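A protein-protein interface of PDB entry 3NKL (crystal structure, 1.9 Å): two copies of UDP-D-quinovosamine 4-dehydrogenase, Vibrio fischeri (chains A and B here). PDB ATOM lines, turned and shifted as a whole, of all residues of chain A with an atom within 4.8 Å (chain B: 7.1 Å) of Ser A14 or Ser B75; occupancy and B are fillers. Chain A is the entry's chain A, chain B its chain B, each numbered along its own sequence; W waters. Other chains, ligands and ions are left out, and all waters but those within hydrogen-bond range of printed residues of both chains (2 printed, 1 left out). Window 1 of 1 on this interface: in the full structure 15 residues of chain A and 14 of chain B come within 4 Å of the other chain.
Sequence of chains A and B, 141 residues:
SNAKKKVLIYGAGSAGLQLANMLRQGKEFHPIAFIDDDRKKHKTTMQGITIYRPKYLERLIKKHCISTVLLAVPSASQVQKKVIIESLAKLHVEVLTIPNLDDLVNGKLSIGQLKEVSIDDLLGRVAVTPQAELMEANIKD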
ATOM      1  N   ALA A  12     -25.568 -16.337  22.415  1.00  0.00           N
ATOM      2  CA  ALA A  12     -25.438 -16.574  23.862  1.00  0.00           C
ATOM      3  C   ALA A  12     -24.013 -16.257  24.350  1.00  0.00           C
ATOM      4  O   ALA A  12     -23.452 -16.972  25.194  1.00  0.00           O
ATOM      5  CB  ALA A  12     -25.828 -18.000  24.223  1.00  0.00           C
ATOM      6  N   GLY A  13     -23.431 -15.198  23.799  1.00  0.00           N
ATOM      7  CA  GLY A  13     -22.147 -14.686  24.272  1.00  0.00           C
ATOM      8  C   GLY A  13     -22.450 -13.716  25.410  1.00  0.00           C
ATOM      9  O   GLY A  13     -23.562 -13.731  25.965  1.00  0.00           O
ATOM     10  N   SER A  14     -21.494 -12.846  25.748  1.00  0.00           N
ATOM     11  CA  SER A  14     -21.665 -11.965  26.901  1.00  0.00           C
ATOM     12  C   SER A  14     -22.877 -11.070  26.703  1.00  0.00           C
ATOM     13  O   SER A  14     -23.699 -10.929  27.590  1.00  0.00           O
ATOM     14  CB  SER A  14     -20.411 -11.103  27.138  1.00  0.00           C
ATOM     15  OG  SER A  14     -20.653 -10.225  28.224  1.00  0.00           O
ATOM     16  N   ALA A  15     -22.976 -10.454  25.529  1.00  0.00           N
ATOM     17  CA  ALA A  15     -24.072  -9.530  25.256  1.00  0.00           C
ATOM     18  C   ALA A  15     -25.443 -10.191  25.358  1.00  0.00           C
ATOM     19  O   ALA A  15     -26.350  -9.648  25.990  1.00  0.00           O
ATOM     20  CB  ALA A  15     -23.884  -8.852  23.880  1.00  0.00           C
ATOM     21  N   GLY A  16     -25.603 -11.351  24.723  1.00  0.00           N
ATOM     22  CA  GLY A  16     -26.877 -12.065  24.733  1.00  0.00           C
ATOM     23  C   GLY A  16     -27.315 -12.476  26.136  1.00  0.00           C
ATOM     24  O   GLY A  16     -28.490 -12.345  26.489  1.00  0.00           O
ATOM     25  N   LEU A  17     -26.375 -12.966  26.940  1.00  0.00           N
ATOM     26  CA  LEU A  17     -26.710 -13.400  28.291  1.00  0.00           C
ATOM     27  C   LEU A  17     -27.121 -12.176  29.104  1.00  0.00           C
ATOM     28  O   LEU A  17     -28.088 -12.227  29.865  1.00  0.00           O
ATOM     29  CB  LEU A  17     -25.535 -14.143  28.965  1.00  0.00           C
ATOM     30  CG  LEU A  17     -25.039 -15.446  28.309  1.00  0.00           C
ATOM     31  CD1 LEU A  17     -24.060 -16.197  29.201  1.00  0.00           C
ATOM     32  CD2 LEU A  17     -26.206 -16.372  27.961  1.00  0.00           C
ATOM     33  N   GLN A  18     -26.391 -11.073  28.936  1.00  0.00           N
ATOM     34  CA  GLN A  18     -26.738  -9.848  29.647  1.00  0.00           C
ATOM     35  C   GLN A  18     -28.117  -9.371  29.199  1.00  0.00           C
ATOM     36  O   GLN A  18     -28.911  -8.909  30.016  1.00  0.00           O
ATOM     37  CB  GLN A  18     -25.692  -8.758  29.429  1.00  0.00           C
ATOM     38  CG  GLN A  18     -24.329  -9.105  30.050  1.00  0.00           C
ATOM     39  CD  GLN A  18     -23.395  -7.932  29.959  1.00  0.00           C
ATOM     40  OE1 GLN A  18     -23.729  -6.841  30.405  1.00  0.00           O
ATOM     41  NE2 GLN A  18     -22.238  -8.138  29.366  1.00  0.00           N
ATOM     42  N   LYS A  41     -21.946 -25.039  23.012  1.00  0.00           N
ATOM     43  CA  LYS A  41     -23.034 -24.551  23.877  1.00  0.00           C
ATOM     44  C   LYS A  41     -24.373 -25.228  23.607  1.00  0.00           C
ATOM     45  O   LYS A  41     -25.358 -24.978  24.319  1.00  0.00           O
ATOM     46  CB  LYS A  41     -23.215 -23.040  23.714  1.00  0.00           C
ATOM     47  CG  LYS A  41     -21.975 -22.236  24.069  1.00  0.00           C
ATOM     48  CD  LYS A  41     -22.228 -20.744  23.988  1.00  0.00           C
ATOM     49  CE  LYS A  41     -20.985 -20.016  24.520  1.00  0.00           C
ATOM     50  NZ  LYS A  41     -21.143 -18.550  24.518  1.00  0.00           N
ATOM     51  N   MET A  46     -27.949 -21.490  30.273  1.00  0.00           N
ATOM     52  CA  MET A  46     -27.401 -20.265  30.864  1.00  0.00           C
ATOM     53  C   MET A  46     -28.569 -19.310  31.073  1.00  0.00           C
ATOM     54  O   MET A  46     -29.527 -19.356  30.313  1.00  0.00           O
ATOM     55  CB  MET A  46     -26.358 -19.594  29.938  1.00  0.00           C
ATOM     56  CG  MET A  46     -25.064 -20.392  29.700  1.00  0.00           C
ATOM     57  SD  MET A  46     -24.007 -20.661  31.367  1.00  0.00           S
ATOM     58  CE  MET A  46     -22.980 -18.997  31.377  1.00  0.00           C
ATOM     59  N   GLY B  13     -14.616 -11.865  22.423  1.00  0.00           N
ATOM     60  CA  GLY B  13     -15.958 -11.341  22.211  1.00  0.00           C
ATOM     61  C   GLY B  13     -16.002  -9.941  22.791  1.00  0.00           C
ATOM     62  O   GLY B  13     -14.962  -9.368  23.117  1.00  0.00           O
ATOM     63  N   SER B  14     -17.201  -9.392  22.952  1.00  0.00           N
ATOM     64  CA  SER B  14     -17.329  -8.039  23.486  1.00  0.00           C
ATOM     65  C   SER B  14     -16.677  -7.834  24.857  1.00  0.00           C
ATOM     66  O   SER B  14     -16.225  -6.734  25.153  1.00  0.00           O
ATOM     67  CB  SER B  14     -18.798  -7.605  23.543  1.00  0.00           C
ATOM     68  OG  SER B  14     -19.501  -8.338  24.547  1.00  0.00           O
ATOM     69  N   ALA B  15     -16.658  -8.855  25.710  1.00  0.00           N
ATOM     70  CA  ALA B  15     -16.045  -8.688  27.034  1.00  0.00           C
ATOM     71  C   ALA B  15     -14.549  -8.539  26.922  1.00  0.00           C
ATOM     72  O   ALA B  15     -13.980  -7.641  27.530  1.00  0.00           O
ATOM     73  CB  ALA B  15     -16.395  -9.870  27.980  1.00  0.00           C
ATOM     74  N   GLY B  16     -13.908  -9.416  26.158  1.00  0.00           N
ATOM     75  CA  GLY B  16     -12.454  -9.381  26.013  1.00  0.00           C
ATOM     76  C   GLY B  16     -11.978  -8.104  25.331  1.00  0.00           C
ATOM     77  O   GLY B  16     -10.920  -7.547  25.641  1.00  0.00           O
ATOM     78  N   GLN B  18     -13.515  -5.155  25.524  1.00  0.00           N
ATOM     79  CA  GLN B  18     -13.576  -4.081  26.509  1.00  0.00           C
ATOM     80  C   GLN B  18     -12.423  -4.182  27.489  1.00  0.00           C
ATOM     81  O   GLN B  18     -11.805  -3.174  27.843  1.00  0.00           O
ATOM     82  CB  GLN B  18     -14.898  -4.112  27.272  1.00  0.00           C
ATOM     83  CG  GLN B  18     -16.104  -3.836  26.426  1.00  0.00           C
ATOM     84  CD  GLN B  18     -17.353  -3.887  27.263  1.00  0.00           C
ATOM     85  OE1 GLN B  18     -17.603  -2.981  28.056  1.00  0.00           O
ATOM     86  NE2 GLN B  18     -18.114  -4.971  27.141  1.00  0.00           N
ATOM     87  N   ALA B  72     -11.574 -13.571  29.869  1.00  0.00           N
ATOM     88  CA  ALA B  72     -12.700 -12.694  29.623  1.00  0.00           C
ATOM     89  C   ALA B  72     -13.757 -13.514  28.879  1.00  0.00           C
ATOM     90  O   ALA B  72     -14.116 -13.207  27.736  1.00  0.00           O
ATOM     91  CB  ALA B  72     -12.262 -11.471  28.805  1.00  0.00           C
ATOM     92  N   VAL B  73     -14.224 -14.577  29.539  1.00  0.00           N
ATOM     93  CA  VAL B  73     -15.246 -15.460  28.984  1.00  0.00           C
ATOM     94  C   VAL B  73     -16.411 -15.648  29.957  1.00  0.00           C
ATOM     95  O   VAL B  73     -16.714 -16.766  30.374  1.00  0.00           O
ATOM     96  CB  VAL B  73     -14.669 -16.841  28.626  1.00  0.00           C
ATOM     97  CG1 VAL B  73     -13.823 -16.739  27.350  1.00  0.00           C
ATOM     98  CG2 VAL B  73     -13.856 -17.422  29.804  1.00  0.00           C
ATOM     99  N   PRO B  74     -17.077 -14.544  30.308  1.00  0.00           N
ATOM    100  CA  PRO B  74     -18.208 -14.601  31.247  1.00  0.00           C
ATOM    101  C   PRO B  74     -19.368 -15.462  30.694  1.00  0.00           C
ATOM    102  O   PRO B  74     -20.210 -15.931  31.463  1.00  0.00           O
ATOM    103  CB  PRO B  74     -18.632 -13.128  31.384  1.00  0.00           C
ATOM    104  CG  PRO B  74     -18.110 -12.446  30.143  1.00  0.00           C
ATOM    105  CD  PRO B  74     -16.777 -13.164  29.879  1.00  0.00           C
ATOM    106  N   SER B  75     -19.398 -15.718  29.389  1.00  0.00           N
ATOM    107  CA  SER B  75     -20.516 -16.526  28.871  1.00  0.00           C
ATOM    108  C   SER B  75     -20.203 -18.019  28.827  1.00  0.00           C
ATOM    109  O   SER B  75     -21.012 -18.810  28.366  1.00  0.00           O
ATOM    110  CB  SER B  75     -20.987 -16.043  27.491  1.00  0.00           C
ATOM    111  OG  SER B  75     -20.015 -16.333  26.501  1.00  0.00           O
ATOM    112  N   ALA B  76     -19.017 -18.405  29.277  1.00  0.00           N
ATOM    113  CA  ALA B  76     -18.668 -19.816  29.296  1.00  0.00           C
ATOM    114  C   ALA B  76     -19.376 -20.468  30.480  1.00  0.00           C
ATOM    115  O   ALA B  76     -19.463 -19.874  31.555  1.00  0.00           O
ATOM    116  CB  ALA B  76     -17.117 -19.969  29.433  1.00  0.00           C
ATOM    117  N   SER B  77     -19.867 -21.688  30.284  1.00  0.00           N
ATOM    118  CA  SER B  77     -20.426 -22.473  31.373  1.00  0.00           C
ATOM    119  C   SER B  77     -19.329 -22.734  32.388  1.00  0.00           C
ATOM    120  O   SER B  77     -18.135 -22.616  32.069  1.00  0.00           O
ATOM    121  CB  SER B  77     -20.950 -23.809  30.847  1.00  0.00           C
ATOM    122  OG  SER B  77     -19.861 -24.564  30.338  1.00  0.00           O
ATOM    123  N   GLN B  78     -19.689 -23.065  33.621  1.00  0.00           N
ATOM    124  CA  GLN B  78     -18.631 -23.318  34.604  1.00  0.00           C
ATOM    125  C   GLN B  78     -17.816 -24.527  34.160  1.00  0.00           C
ATOM    126  O   GLN B  78     -16.599 -24.528  34.268  1.00  0.00           O
ATOM    127  CB  GLN B  78     -19.194 -23.500  36.014  1.00  0.00           C
ATOM    128  CG  GLN B  78     -19.624 -22.190  36.655  1.00  0.00           C
ATOM    129  CD  GLN B  78     -18.442 -21.325  37.069  1.00  0.00           C
ATOM    130  OE1 GLN B  78     -18.108 -20.335  36.409  1.00  0.00           O
ATOM    131  NE2 GLN B  78     -17.796 -21.706  38.166  1.00  0.00           N
ATOM    132  N   GLN B  80     -17.055 -25.454  31.145  1.00  0.00           N
ATOM    133  CA  GLN B  80     -16.146 -25.010  30.093  1.00  0.00           C
ATOM    134  C   GLN B  80     -15.052 -24.078  30.632  1.00  0.00           C
ATOM    135  O   GLN B  80     -13.908 -24.116  30.177  1.00  0.00           O
ATOM    136  CB  GLN B  80     -16.939 -24.311  28.986  1.00  0.00           C
ATOM    137  CG  GLN B  80     -16.085 -23.778  27.850  1.00  0.00           C
ATOM    138  CD  GLN B  80     -15.191 -24.842  27.209  1.00  0.00           C
ATOM    139  OE1 GLN B  80     -14.040 -24.568  26.851  1.00  0.00           O
ATOM    140  NE2 GLN B  80     -15.717 -26.053  27.059  1.00  0.00           N
ATOM    141  N   ILE B  98     -11.981 -11.782  34.826  1.00  0.00           N
ATOM    142  CA  ILE B  98     -12.914 -10.680  35.068  1.00  0.00           C
ATOM    143  C   ILE B  98     -14.114 -11.250  35.840  1.00  0.00           C
ATOM    144  O   ILE B  98     -14.231 -12.472  35.976  1.00  0.00           O
ATOM    145  CB  ILE B  98     -13.368 -10.039  33.741  1.00  0.00           C
ATOM    146  CG1 ILE B  98     -14.308 -10.970  32.963  1.00  0.00           C
ATOM    147  CG2 ILE B  98     -12.138  -9.647  32.872  1.00  0.00           C
ATOM    148  CD1 ILE B  98     -14.912 -10.263  31.710  1.00  0.00           C
ATOM    149  N   LEU B 101     -20.771 -13.035  34.849  1.00  0.00           N
ATOM    150  CA  LEU B 101     -21.741 -12.329  34.033  1.00  0.00           C
ATOM    151  C   LEU B 101     -22.739 -11.509  34.851  1.00  0.00           C
ATOM    152  O   LEU B 101     -22.975 -10.334  34.567  1.00  0.00           O
ATOM    153  CB  LEU B 101     -22.492 -13.318  33.133  1.00  0.00           C
ATOM    154  CG  LEU B 101     -23.128 -12.373  32.115  1.00  0.00           C
ATOM    155  CD1 LEU B 101     -22.539 -12.504  30.708  1.00  0.00           C
ATOM    156  CD2 LEU B 101     -24.629 -12.376  32.163  1.00  0.00           C
ATOM    157  N   LEU B 104     -21.562  -8.321  36.091  1.00  0.00           N
ATOM    158  CA  LEU B 104     -21.285  -7.308  35.081  1.00  0.00           C
ATOM    159  C   LEU B 104     -22.555  -6.591  34.644  1.00  0.00           C
ATOM    160  O   LEU B 104     -22.524  -5.425  34.255  1.00  0.00           O
ATOM    161  CB  LEU B 104     -20.658  -7.939  33.851  1.00  0.00           C
ATOM    162  CG  LEU B 104     -19.288  -8.545  34.104  1.00  0.00           C
ATOM    163  CD1 LEU B 104     -18.800  -9.170  32.805  1.00  0.00           C
ATOM    164  CD2 LEU B 104     -18.363  -7.439  34.561  1.00  0.00           C
ATOM    165  N   ILE B 111     -15.509  -4.714  34.572  1.00  0.00           N
ATOM    166  CA  ILE B 111     -14.750  -5.695  33.804  1.00  0.00           C
ATOM    167  C   ILE B 111     -13.258  -5.641  34.150  1.00  0.00           C
ATOM    168  O   ILE B 111     -12.539  -6.637  34.041  1.00  0.00           O
ATOM    169  CB  ILE B 111     -14.973  -5.485  32.283  1.00  0.00           C
ATOM    170  CG1 ILE B 111     -16.411  -5.840  31.915  1.00  0.00           C
ATOM    171  CG2 ILE B 111     -14.075  -6.395  31.452  1.00  0.00           C
ATOM    172  CD1 ILE B 111     -16.701  -5.696  30.439  1.00  0.00           C
HETATM  173  O   HOH W   1     -23.229 -19.123  26.904  1.00  0.00           O
HETATM  174  O   HOH W   2     -20.618  -5.469  28.490  1.00  0.00           O
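O of Ala A12 lies within hydrogen-bond range of NZ of Lys A41. The side-chain hydroxyl (OG) of Ser A14 is in hydrogen-bond range of the side-chain amide nitrogen (NE2) of Gln A18 (2.9 Å). O of Ser B14 sits close to NE2 of Gln B18, at 3.3 Å.
Ser B75 touches Ala A12. Ser B14 touches Ser A14 (OG to CB, 3.9 Å). Pro B74 touches Ser A14 (CG to OG, 3.9 Å). Ser B75 touches Ser A14 (CB to N, 3.7 Å). CD1 of Leu B101 touches O of Ser A14 (3.7 Å). Leu A17 touches Ser B75. Leu A17 touches Leu B101 (CB to CD2, 3.8 Å). Gln A18 touches Leu B101. Ser B75 touches Met A46. CE of Met A46 touches O of Ala B76 (3.6 Å).
Water W1 lies within hydrogen-bond range of O of Ser B75 (2.7 Å), O of Ala A12 (2.8 Å) and NZ of Lys A41 (3.2 Å). Water W2 lies within hydrogen-bond range of NE2 of Gln B18 (2.9 Å) and NE2 of Gln A18 (3.2 Å).
Hydrophobic or aromatic side chains of chain B that line the printed part of chain A: Pro B74 and Leu B101. Of the 9 printed residues of chain A, 7 touch a printed residue of chain B. Among the printed residues, 12 pairs touch across the chains. Among the printed residues, no Asp or Glu carboxylate lies within 4 Å of a Lys or Arg side-chain nitrogen of the other chain.
OG of Ser B75 lies within hydrogen-bond range of NZ of Lys A41 (3.2 Å).
Printed residues of chain B within 4 Å of Ser A14: Ser B14 (3.9 Å), Pro B74 (3.9 Å), Ser B75 (3.7 Å) and Leu B101 (3.7 Å). Printed residues of chain A within 4 Å of Ser B75: Ala A12 (3.5 Å), Gly A13 (3.4 Å), Ser A14 (3.7 Å), Leu A17 (3.5 Å), Lys A41 (3.2 Å) and Met A46 (3.6 Å). Of the printed residues of chain B, Gly A13 touches Ser B75 (3.4 Å). Printed residues of chain B within 4 Å of Gln A18: Leu B101 (3.9 Å). The nearest residue of chain B that does not touch Ser A14 is Ala B15 (4.3 Å).
Ser B14 touches its own counterpart, Ser A14. 5 positions are printed for both chains.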
